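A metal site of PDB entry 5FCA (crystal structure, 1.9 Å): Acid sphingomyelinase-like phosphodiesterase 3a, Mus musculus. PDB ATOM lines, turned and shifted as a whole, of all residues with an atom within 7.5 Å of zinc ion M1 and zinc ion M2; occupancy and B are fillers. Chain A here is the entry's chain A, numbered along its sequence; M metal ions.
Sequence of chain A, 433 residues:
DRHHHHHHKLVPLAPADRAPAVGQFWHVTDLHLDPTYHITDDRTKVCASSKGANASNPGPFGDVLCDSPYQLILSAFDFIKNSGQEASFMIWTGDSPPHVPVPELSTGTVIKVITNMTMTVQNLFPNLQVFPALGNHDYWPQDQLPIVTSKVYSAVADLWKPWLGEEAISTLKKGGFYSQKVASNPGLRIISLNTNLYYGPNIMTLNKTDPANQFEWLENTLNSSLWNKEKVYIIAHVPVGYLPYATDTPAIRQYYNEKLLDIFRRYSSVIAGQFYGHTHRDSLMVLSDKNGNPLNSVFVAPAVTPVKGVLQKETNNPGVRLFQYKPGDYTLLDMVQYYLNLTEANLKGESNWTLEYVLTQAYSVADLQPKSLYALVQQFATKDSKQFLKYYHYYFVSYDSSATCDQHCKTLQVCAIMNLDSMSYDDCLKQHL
Zinc ion M2 is bound by the side-chain carboxylate (OD2) of Asp 30 (2.1 Å), a ring nitrogen (NE2) of His 32 (2.1 Å), a ring nitrogen (NE2) of His 280 (2.2 Å) and the side-chain carboxylate (OD2) of Asp 95 (2.4 Å).
Zinc ion M1 is bound by NE2 of His 237 (2.1 Å), OD1 of Asn 136 (2.1 Å), ND1 of His 278 (2.2 Å) and OD2 of Asp 95 (2.4 Å). Zinc ion M1 has four donor atoms within binding distance.
Within 4 Å of zinc ion M2: Asp 30, His 32, Asp 95 and His 280.
Of the 28 residues printed, 5 come within 4 Å of zinc ion M1. The nearest printed residue that does not touch zinc ion M1 is His 137 (4.4 Å).
N of His 137 sits at hydrogen-bond distance from OD1 of Asp 95, at 2.8 Å. O of Asp 95 lies within hydrogen-bond range of N of Leu 31 (3.4 Å). The backbone carbonyl oxygen (O) of Thr 93 sits at hydrogen-bond distance from a ring nitrogen (ND1) of His 237, 2.7 Å away. The backbone NH (N) of Gly 277 is in hydrogen-bond range of the backbone carbonyl oxygen (O) of His 237, at 3.1 Å. The side-chain carboxylate (OD1) of Asp 30 sits at hydrogen-bond distance from the side-chain hydroxyl (OG1) of Thr 29 (2.7 Å). The backbone NH (N) of Asp 95 lies within hydrogen-bond range of the side-chain carboxylate (OD2) of Asp 138, at 2.9 Å. A ring nitrogen (ND1) of His 32 sits at hydrogen-bond distance from the backbone carbonyl oxygen of Pro 97 (2.8 Å). N of His 278 sits at hydrogen-bond distance from OD1 of Asp 30 (2.9 Å).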
ATOM      1  N   THR A  29       5.257  -4.569  23.876  1.00  0.00           N
ATOM      2  CA  THR A  29       5.939  -4.319  22.606  1.00  0.00           C
ATOM      3  C   THR A  29       5.858  -2.853  22.220  1.00  0.00           C
ATOM      4  O   THR A  29       4.936  -2.151  22.626  1.00  0.00           O
ATOM      5  CB  THR A  29       5.370  -5.206  21.473  1.00  0.00           C
ATOM      6  OG1 THR A  29       6.238  -5.106  20.327  1.00  0.00           O
ATOM      7  CG2 THR A  29       3.976  -4.777  21.056  1.00  0.00           C
ATOM      8  N   ASP A  30       6.873  -2.393  21.494  1.00  0.00           N
ATOM      9  CA  ASP A  30       6.852  -1.099  20.845  1.00  0.00           C
ATOM     10  C   ASP A  30       6.645   0.040  21.859  1.00  0.00           C
ATOM     11  O   ASP A  30       5.686   0.821  21.804  1.00  0.00           O
ATOM     12  CB  ASP A  30       5.781  -1.079  19.759  1.00  0.00           C
ATOM     13  CG  ASP A  30       6.131  -2.008  18.594  1.00  0.00           C
ATOM     14  OD1 ASP A  30       5.629  -3.154  18.583  1.00  0.00           O
ATOM     15  OD2 ASP A  30       6.891  -1.555  17.704  1.00  0.00           O
ATOM     16  N   LEU A  31       7.599   0.128  22.778  1.00  0.00           N
ATOM     17  CA  LEU A  31       7.547   1.116  23.845  1.00  0.00           C
ATOM     18  C   LEU A  31       7.879   2.508  23.334  1.00  0.00           C
ATOM     19  O   LEU A  31       7.286   3.507  23.783  1.00  0.00           O
ATOM     20  CB  LEU A  31       8.516   0.702  24.963  1.00  0.00           C
ATOM     21  CG  LEU A  31       8.292  -0.671  25.584  1.00  0.00           C
ATOM     22  CD1 LEU A  31       9.420  -0.993  26.558  1.00  0.00           C
ATOM     23  CD2 LEU A  31       6.960  -0.692  26.272  1.00  0.00           C
ATOM     24  N   HIS A  32       8.864   2.607  22.432  1.00  0.00           N
ATOM     25  CA  HIS A  32       9.219   3.840  21.744  1.00  0.00           C
ATOM     26  C   HIS A  32       9.302   5.027  22.711  1.00  0.00           C
ATOM     27  O   HIS A  32       8.581   6.025  22.608  1.00  0.00           O
ATOM     28  CB  HIS A  32       8.223   4.111  20.619  1.00  0.00           C
ATOM     29  CG  HIS A  32       8.355   3.185  19.455  1.00  0.00           C
ATOM     30  ND1 HIS A  32       9.425   3.231  18.594  1.00  0.00           N
ATOM     31  CD2 HIS A  32       7.529   2.220  18.971  1.00  0.00           C
ATOM     32  CE1 HIS A  32       9.266   2.338  17.638  1.00  0.00           C
ATOM     33  NE2 HIS A  32       8.116   1.720  17.845  1.00  0.00           N
ATOM     34  N   ASP A  67       5.757   9.953  20.486  1.00  0.00           N
ATOM     35  CA  ASP A  67       6.084   8.679  21.080  1.00  0.00           C
ATOM     36  C   ASP A  67       5.911   8.783  22.599  1.00  0.00           C
ATOM     37  O   ASP A  67       5.422   9.792  23.132  1.00  0.00           O
ATOM     38  CB  ASP A  67       7.467   8.262  20.631  1.00  0.00           C
ATOM     39  CG  ASP A  67       7.392   7.325  19.425  1.00  0.00           C
ATOM     40  OD1 ASP A  67       6.415   6.546  19.344  1.00  0.00           O
ATOM     41  OD2 ASP A  67       8.289   7.397  18.556  1.00  0.00           O
ATOM     42  N   THR A  93       8.838  -7.629  22.511  1.00  0.00           N
ATOM     43  CA  THR A  93       9.200  -7.789  21.113  1.00  0.00           C
ATOM     44  C   THR A  93       9.655  -6.492  20.461  1.00  0.00           C
ATOM     45  O   THR A  93       9.442  -6.290  19.271  1.00  0.00           O
ATOM     46  CB  THR A  93       8.075  -8.443  20.327  1.00  0.00           C
ATOM     47  OG1 THR A  93       6.848  -7.780  20.551  1.00  0.00           O
ATOM     48  CG2 THR A  93       7.918  -9.901  20.761  1.00  0.00           C
ATOM     49  N   GLY A  94      10.303  -5.600  21.207  1.00  0.00           N
ATOM     50  CA  GLY A  94      11.277  -4.689  20.607  1.00  0.00           C
ATOM     51  C   GLY A  94      10.728  -3.301  20.347  1.00  0.00           C
ATOM     52  O   GLY A  94       9.594  -2.976  20.669  1.00  0.00           O
ATOM     53  N   ASP A  95      11.617  -2.468  19.781  1.00  0.00           N
ATOM     54  CA  ASP A  95      11.391  -1.089  19.300  1.00  0.00           C
ATOM     55  C   ASP A  95      11.374  -0.024  20.410  1.00  0.00           C
ATOM     56  O   ASP A  95      10.330   0.529  20.775  1.00  0.00           O
ATOM     57  CB  ASP A  95      10.128  -1.042  18.444  1.00  0.00           C
ATOM     58  CG  ASP A  95      10.436  -0.895  16.959  1.00  0.00           C
ATOM     59  OD1 ASP A  95      11.576  -1.138  16.487  1.00  0.00           O
ATOM     60  OD2 ASP A  95       9.493  -0.500  16.252  1.00  0.00           O
ATOM     61  N   SER A  96      12.550   0.332  20.925  1.00  0.00           N
ATOM     62  CA  SER A  96      12.642   1.186  22.111  1.00  0.00           C
ATOM     63  C   SER A  96      12.958   2.636  21.772  1.00  0.00           C
ATOM     64  O   SER A  96      12.404   3.531  22.409  1.00  0.00           O
ATOM     65  CB  SER A  96      13.688   0.598  23.084  1.00  0.00           C
ATOM     66  OG  SER A  96      13.172  -0.570  23.712  1.00  0.00           O
ATOM     67  N   PRO A  97      13.844   2.937  20.842  1.00  0.00           N
ATOM     68  CA  PRO A  97      14.053   4.335  20.488  1.00  0.00           C
ATOM     69  C   PRO A  97      12.831   4.926  19.826  1.00  0.00           C
ATOM     70  O   PRO A  97      11.946   4.186  19.336  1.00  0.00           O
ATOM     71  CB  PRO A  97      15.246   4.278  19.518  1.00  0.00           C
ATOM     72  CG  PRO A  97      15.932   3.035  19.870  1.00  0.00           C
ATOM     73  CD  PRO A  97      14.860   2.075  20.225  1.00  0.00           C
ATOM     74  N   HIS A  99      10.618   7.698  17.176  1.00  0.00           N
ATOM     75  CA  HIS A  99      10.582   8.045  15.761  1.00  0.00           C
ATOM     76  C   HIS A  99      11.145   9.441  15.570  1.00  0.00           C
ATOM     77  O   HIS A  99      10.404  10.430  15.512  1.00  0.00           O
ATOM     78  CB  HIS A  99       9.150   7.948  15.234  1.00  0.00           C
ATOM     79  CG  HIS A  99       8.617   6.544  15.180  1.00  0.00           C
ATOM     80  ND1 HIS A  99       8.044   5.927  16.259  1.00  0.00           N
ATOM     81  CD2 HIS A  99       8.607   5.647  14.169  1.00  0.00           C
ATOM     82  CE1 HIS A  99       7.663   4.703  15.919  1.00  0.00           C
ATOM     83  NE2 HIS A  99       7.997   4.517  14.648  1.00  0.00           N
ATOM     84  N   LEU A 134      14.715  -7.959  19.112  1.00  0.00           N
ATOM     85  CA  LEU A 134      15.072  -6.653  18.595  1.00  0.00           C
ATOM     86  C   LEU A 134      14.039  -6.180  17.583  1.00  0.00           C
ATOM     87  O   LEU A 134      13.463  -6.963  16.825  1.00  0.00           O
ATOM     88  CB  LEU A 134      16.454  -6.689  17.941  1.00  0.00           C
ATOM     89  CG  LEU A 134      17.642  -6.961  18.841  1.00  0.00           C
ATOM     90  CD1 LEU A 134      18.831  -7.394  17.985  1.00  0.00           C
ATOM     91  CD2 LEU A 134      17.966  -5.684  19.636  1.00  0.00           C
ATOM     92  N   GLY A 135      13.807  -4.858  17.592  1.00  0.00           N
ATOM     93  CA  GLY A 135      12.948  -4.186  16.654  1.00  0.00           C
ATOM     94  C   GLY A 135      13.742  -3.399  15.644  1.00  0.00           C
ATOM     95  O   GLY A 135      14.952  -3.235  15.756  1.00  0.00           O
ATOM     96  N   ASN A 136      13.048  -2.928  14.586  1.00  0.00           N
ATOM     97  CA  ASN A 136      13.779  -2.271  13.510  1.00  0.00           C
ATOM     98  C   ASN A 136      14.326  -0.915  13.943  1.00  0.00           C
ATOM     99  O   ASN A 136      15.286  -0.414  13.333  1.00  0.00           O
ATOM    100  CB  ASN A 136      12.893  -2.114  12.268  1.00  0.00           C
ATOM    101  CG  ASN A 136      11.602  -1.398  12.561  1.00  0.00           C
ATOM    102  OD1 ASN A 136      10.800  -1.853  13.354  1.00  0.00           O
ATOM    103  ND2 ASN A 136      11.405  -0.262  11.922  1.00  0.00           N
ATOM    104  N   HIS A 137      13.775  -0.335  14.989  1.00  0.00           N
ATOM    105  CA  HIS A 137      14.302   0.888  15.576  1.00  0.00           C
ATOM    106  C   HIS A 137      15.391   0.635  16.602  1.00  0.00           C
ATOM    107  O   HIS A 137      15.995   1.602  17.096  1.00  0.00           O
ATOM    108  CB  HIS A 137      13.145   1.661  16.212  1.00  0.00           C
ATOM    109  CG  HIS A 137      12.303   2.375  15.212  1.00  0.00           C
ATOM    110  ND1 HIS A 137      12.702   3.544  14.621  1.00  0.00           N
ATOM    111  CD2 HIS A 137      11.089   2.065  14.689  1.00  0.00           C
ATOM    112  CE1 HIS A 137      11.763   3.944  13.783  1.00  0.00           C
ATOM    113  NE2 HIS A 137      10.767   3.078  13.811  1.00  0.00           N
ATOM    114  N   ASP A 138      15.688  -0.624  16.916  1.00  0.00           N
ATOM    115  CA  ASP A 138      16.732  -0.965  17.882  1.00  0.00           C
ATOM    116  C   ASP A 138      18.099  -1.039  17.235  1.00  0.00           C
ATOM    117  O   ASP A 138      18.872  -1.962  17.500  1.00  0.00           O
ATOM    118  CB  ASP A 138      16.363  -2.286  18.580  1.00  0.00           C
ATOM    119  CG  ASP A 138      15.136  -2.128  19.476  1.00  0.00           C
ATOM    120  OD1 ASP A 138      14.858  -0.990  19.897  1.00  0.00           O
ATOM    121  OD2 ASP A 138      14.452  -3.131  19.767  1.00  0.00           O
ATOM    122  N   ASP A 143      16.456   0.330  10.988  1.00  0.00           N
ATOM    123  CA  ASP A 143      16.157  -0.688   9.987  1.00  0.00           C
ATOM    124  C   ASP A 143      17.388  -1.388   9.412  1.00  0.00           C
ATOM    125  O   ASP A 143      17.246  -2.411   8.740  1.00  0.00           O
ATOM    126  CB  ASP A 143      15.376  -0.090   8.803  1.00  0.00           C
ATOM    127  CG  ASP A 143      14.146   0.710   9.208  1.00  0.00           C
ATOM    128  OD1 ASP A 143      13.471   0.373  10.195  1.00  0.00           O
ATOM    129  OD2 ASP A 143      13.846   1.695   8.503  1.00  0.00           O
ATOM    130  N   ASN A 196      13.746  -8.327  11.501  1.00  0.00           N
ATOM    131  CA  ASN A 196      14.257  -7.140  10.853  1.00  0.00           C
ATOM    132  C   ASN A 196      15.262  -7.457   9.756  1.00  0.00           C
ATOM    133  O   ASN A 196      15.494  -6.598   8.891  1.00  0.00           O
ATOM    134  CB  ASN A 196      14.905  -6.233  11.882  1.00  0.00           C
ATOM    135  CG  ASN A 196      14.035  -6.028  13.053  1.00  0.00           C
ATOM    136  OD1 ASN A 196      13.019  -5.339  12.965  1.00  0.00           O
ATOM    137  ND2 ASN A 196      14.335  -6.716  14.142  1.00  0.00           N
ATOM    138  N   TYR A 199      13.108  -7.246   6.671  1.00  0.00           N
ATOM    139  CA  TYR A 199      12.261  -6.069   6.545  1.00  0.00           C
ATOM    140  C   TYR A 199      12.709  -5.220   5.364  1.00  0.00           C
ATOM    141  O   TYR A 199      13.908  -5.011   5.144  1.00  0.00           O
ATOM    142  CB  TYR A 199      12.305  -5.293   7.872  1.00  0.00           C
ATOM    143  CG  TYR A 199      11.376  -4.095   8.003  1.00  0.00           C
ATOM    144  CD1 TYR A 199      10.050  -4.174   7.664  1.00  0.00           C
ATOM    145  CD2 TYR A 199      11.849  -2.893   8.516  1.00  0.00           C
ATOM    146  CE1 TYR A 199       9.215  -3.095   7.804  1.00  0.00           C
ATOM    147  CE2 TYR A 199      11.011  -1.790   8.649  1.00  0.00           C
ATOM    148  CZ  TYR A 199       9.693  -1.907   8.283  1.00  0.00           C
ATOM    149  OH  TYR A 199       8.814  -0.832   8.379  1.00  0.00           O
ATOM    150  N   HIS A 237       9.835  -9.197  16.089  1.00  0.00           N
ATOM    151  CA  HIS A 237       9.270  -7.870  15.922  1.00  0.00           C
ATOM    152  C   HIS A 237       8.346  -7.778  14.717  1.00  0.00           C
ATOM    153  O   HIS A 237       7.127  -7.686  14.875  1.00  0.00           O
ATOM    154  CB  HIS A 237      10.366  -6.820  15.798  1.00  0.00           C
ATOM    155  CG  HIS A 237       9.825  -5.432  15.855  1.00  0.00           C
ATOM    156  ND1 HIS A 237       9.053  -4.985  16.896  1.00  0.00           N
ATOM    157  CD2 HIS A 237       9.883  -4.407  14.965  1.00  0.00           C
ATOM    158  CE1 HIS A 237       8.671  -3.741  16.663  1.00  0.00           C
ATOM    159  NE2 HIS A 237       9.170  -3.373  15.500  1.00  0.00           N
ATOM    160  N   VAL A 238       8.902  -7.754  13.501  1.00  0.00           N
ATOM    161  CA  VAL A 238       8.065  -7.655  12.293  1.00  0.00           C
ATOM    162  C   VAL A 238       7.366  -8.982  12.053  1.00  0.00           C
ATOM    163  O   VAL A 238       8.029 -10.046  12.060  1.00  0.00           O
ATOM    164  CB  VAL A 238       8.913  -7.282  11.080  1.00  0.00           C
ATOM    165  CG1 VAL A 238       7.980  -7.038   9.878  1.00  0.00           C
ATOM    166  CG2 VAL A 238       9.764  -6.072  11.355  1.00  0.00           C
ATOM    167  N   GLY A 277       5.030  -7.900  17.086  1.00  0.00           N
ATOM    168  CA  GLY A 277       4.558  -6.530  17.228  1.00  0.00           C
ATOM    169  C   GLY A 277       4.727  -5.732  15.963  1.00  0.00           C
ATOM    170  O   GLY A 277       4.258  -6.115  14.898  1.00  0.00           O
ATOM    171  N   HIS A 278       5.446  -4.628  16.056  1.00  0.00           N
ATOM    172  CA  HIS A 278       5.795  -3.756  14.946  1.00  0.00           C
ATOM    173  C   HIS A 278       4.628  -2.992  14.321  1.00  0.00           C
ATOM    174  O   HIS A 278       4.800  -1.831  13.925  1.00  0.00           O
ATOM    175  CB  HIS A 278       6.507  -4.519  13.826  1.00  0.00           C
ATOM    176  CG  HIS A 278       6.810  -3.684  12.653  1.00  0.00           C
ATOM    177  ND1 HIS A 278       7.790  -2.708  12.652  1.00  0.00           N
ATOM    178  CD2 HIS A 278       6.262  -3.654  11.409  1.00  0.00           C
ATOM    179  CE1 HIS A 278       7.845  -2.136  11.469  1.00  0.00           C
ATOM    180  NE2 HIS A 278       6.932  -2.688  10.701  1.00  0.00           N
ATOM    181  N   THR A 279       3.462  -3.608  14.196  1.00  0.00           N
ATOM    182  CA  THR A 279       2.375  -2.893  13.520  1.00  0.00           C
ATOM    183  C   THR A 279       1.675  -1.898  14.422  1.00  0.00           C
ATOM    184  O   THR A 279       0.959  -1.037  13.925  1.00  0.00           O
ATOM    185  CB  THR A 279       1.312  -3.854  12.994  1.00  0.00           C
ATOM    186  OG1 THR A 279       0.593  -4.406  14.085  1.00  0.00           O
ATOM    187  CG2 THR A 279       1.872  -4.991  12.166  1.00  0.00           C
ATOM    188  N   HIS A 280       1.816  -2.032  15.738  1.00  0.00           N
ATOM    189  CA  HIS A 280       1.158  -1.170  16.723  1.00  0.00           C
ATOM    190  C   HIS A 280      -0.343  -1.365  16.751  1.00  0.00           C
ATOM    191  O   HIS A 280      -1.068  -0.499  17.224  1.00  0.00           O
ATOM    192  CB  HIS A 280       1.474   0.311  16.480  1.00  0.00           C
ATOM    193  CG  HIS A 280       2.920   0.669  16.650  1.00  0.00           C
ATOM    194  ND1 HIS A 280       3.341   1.966  16.844  1.00  0.00           N
ATOM    195  CD2 HIS A 280       4.038  -0.096  16.647  1.00  0.00           C
ATOM    196  CE1 HIS A 280       4.665   1.985  16.947  1.00  0.00           C
ATOM    197  NE2 HIS A 280       5.107   0.750  16.818  1.00  0.00           N
ATOM    198  N   ALA A 303       0.906  -1.582  20.456  1.00  0.00           N
ATOM    199  CA  ALA A 303       2.030  -0.908  21.077  1.00  0.00           C
ATOM    200  C   ALA A 303       1.590  -0.156  22.332  1.00  0.00           C
ATOM    201  O   ALA A 303       0.430   0.223  22.496  1.00  0.00           O
ATOM    202  CB  ALA A 303       2.666   0.056  20.095  1.00  0.00           C
ATOM    203  N   THR A 305       3.266   2.811  22.823  1.00  0.00           N
ATOM    204  CA  THR A 305       3.235   4.133  22.219  1.00  0.00           C
ATOM    205  C   THR A 305       1.952   4.319  21.425  1.00  0.00           C
ATOM    206  O   THR A 305       1.432   3.354  20.848  1.00  0.00           O
ATOM    207  CB  THR A 305       4.432   4.368  21.309  1.00  0.00           C
ATOM    208  OG1 THR A 305       4.429   5.739  20.918  1.00  0.00           O
ATOM    209  CG2 THR A 305       4.367   3.494  20.042  1.00  0.00           C
ATOM    210  N   VAL A 307       1.815   6.704  18.979  1.00  0.00           N
ATOM    211  CA  VAL A 307       2.226   7.657  17.958  1.00  0.00           C
ATOM    212  C   VAL A 307       1.575   7.347  16.620  1.00  0.00           C
ATOM    213  O   VAL A 307       1.366   6.183  16.259  1.00  0.00           O
ATOM    214  CB  VAL A 307       3.751   7.660  17.848  1.00  0.00           C
ATOM    215  CG1 VAL A 307       4.254   6.357  17.162  1.00  0.00           C
ATOM    216  CG2 VAL A 307       4.241   8.905  17.123  1.00  0.00           C
HETATM  217 ZN    ZN M   1       8.912  -1.689  14.269  1.00  0.00          ZN
HETATM  218 ZN    ZN M   2       7.208   0.219  16.701  1.00  0.00          ZN
HETATM  219 ZN    ZN M   3       8.328   2.295  12.995  1.00  0.00          ZN
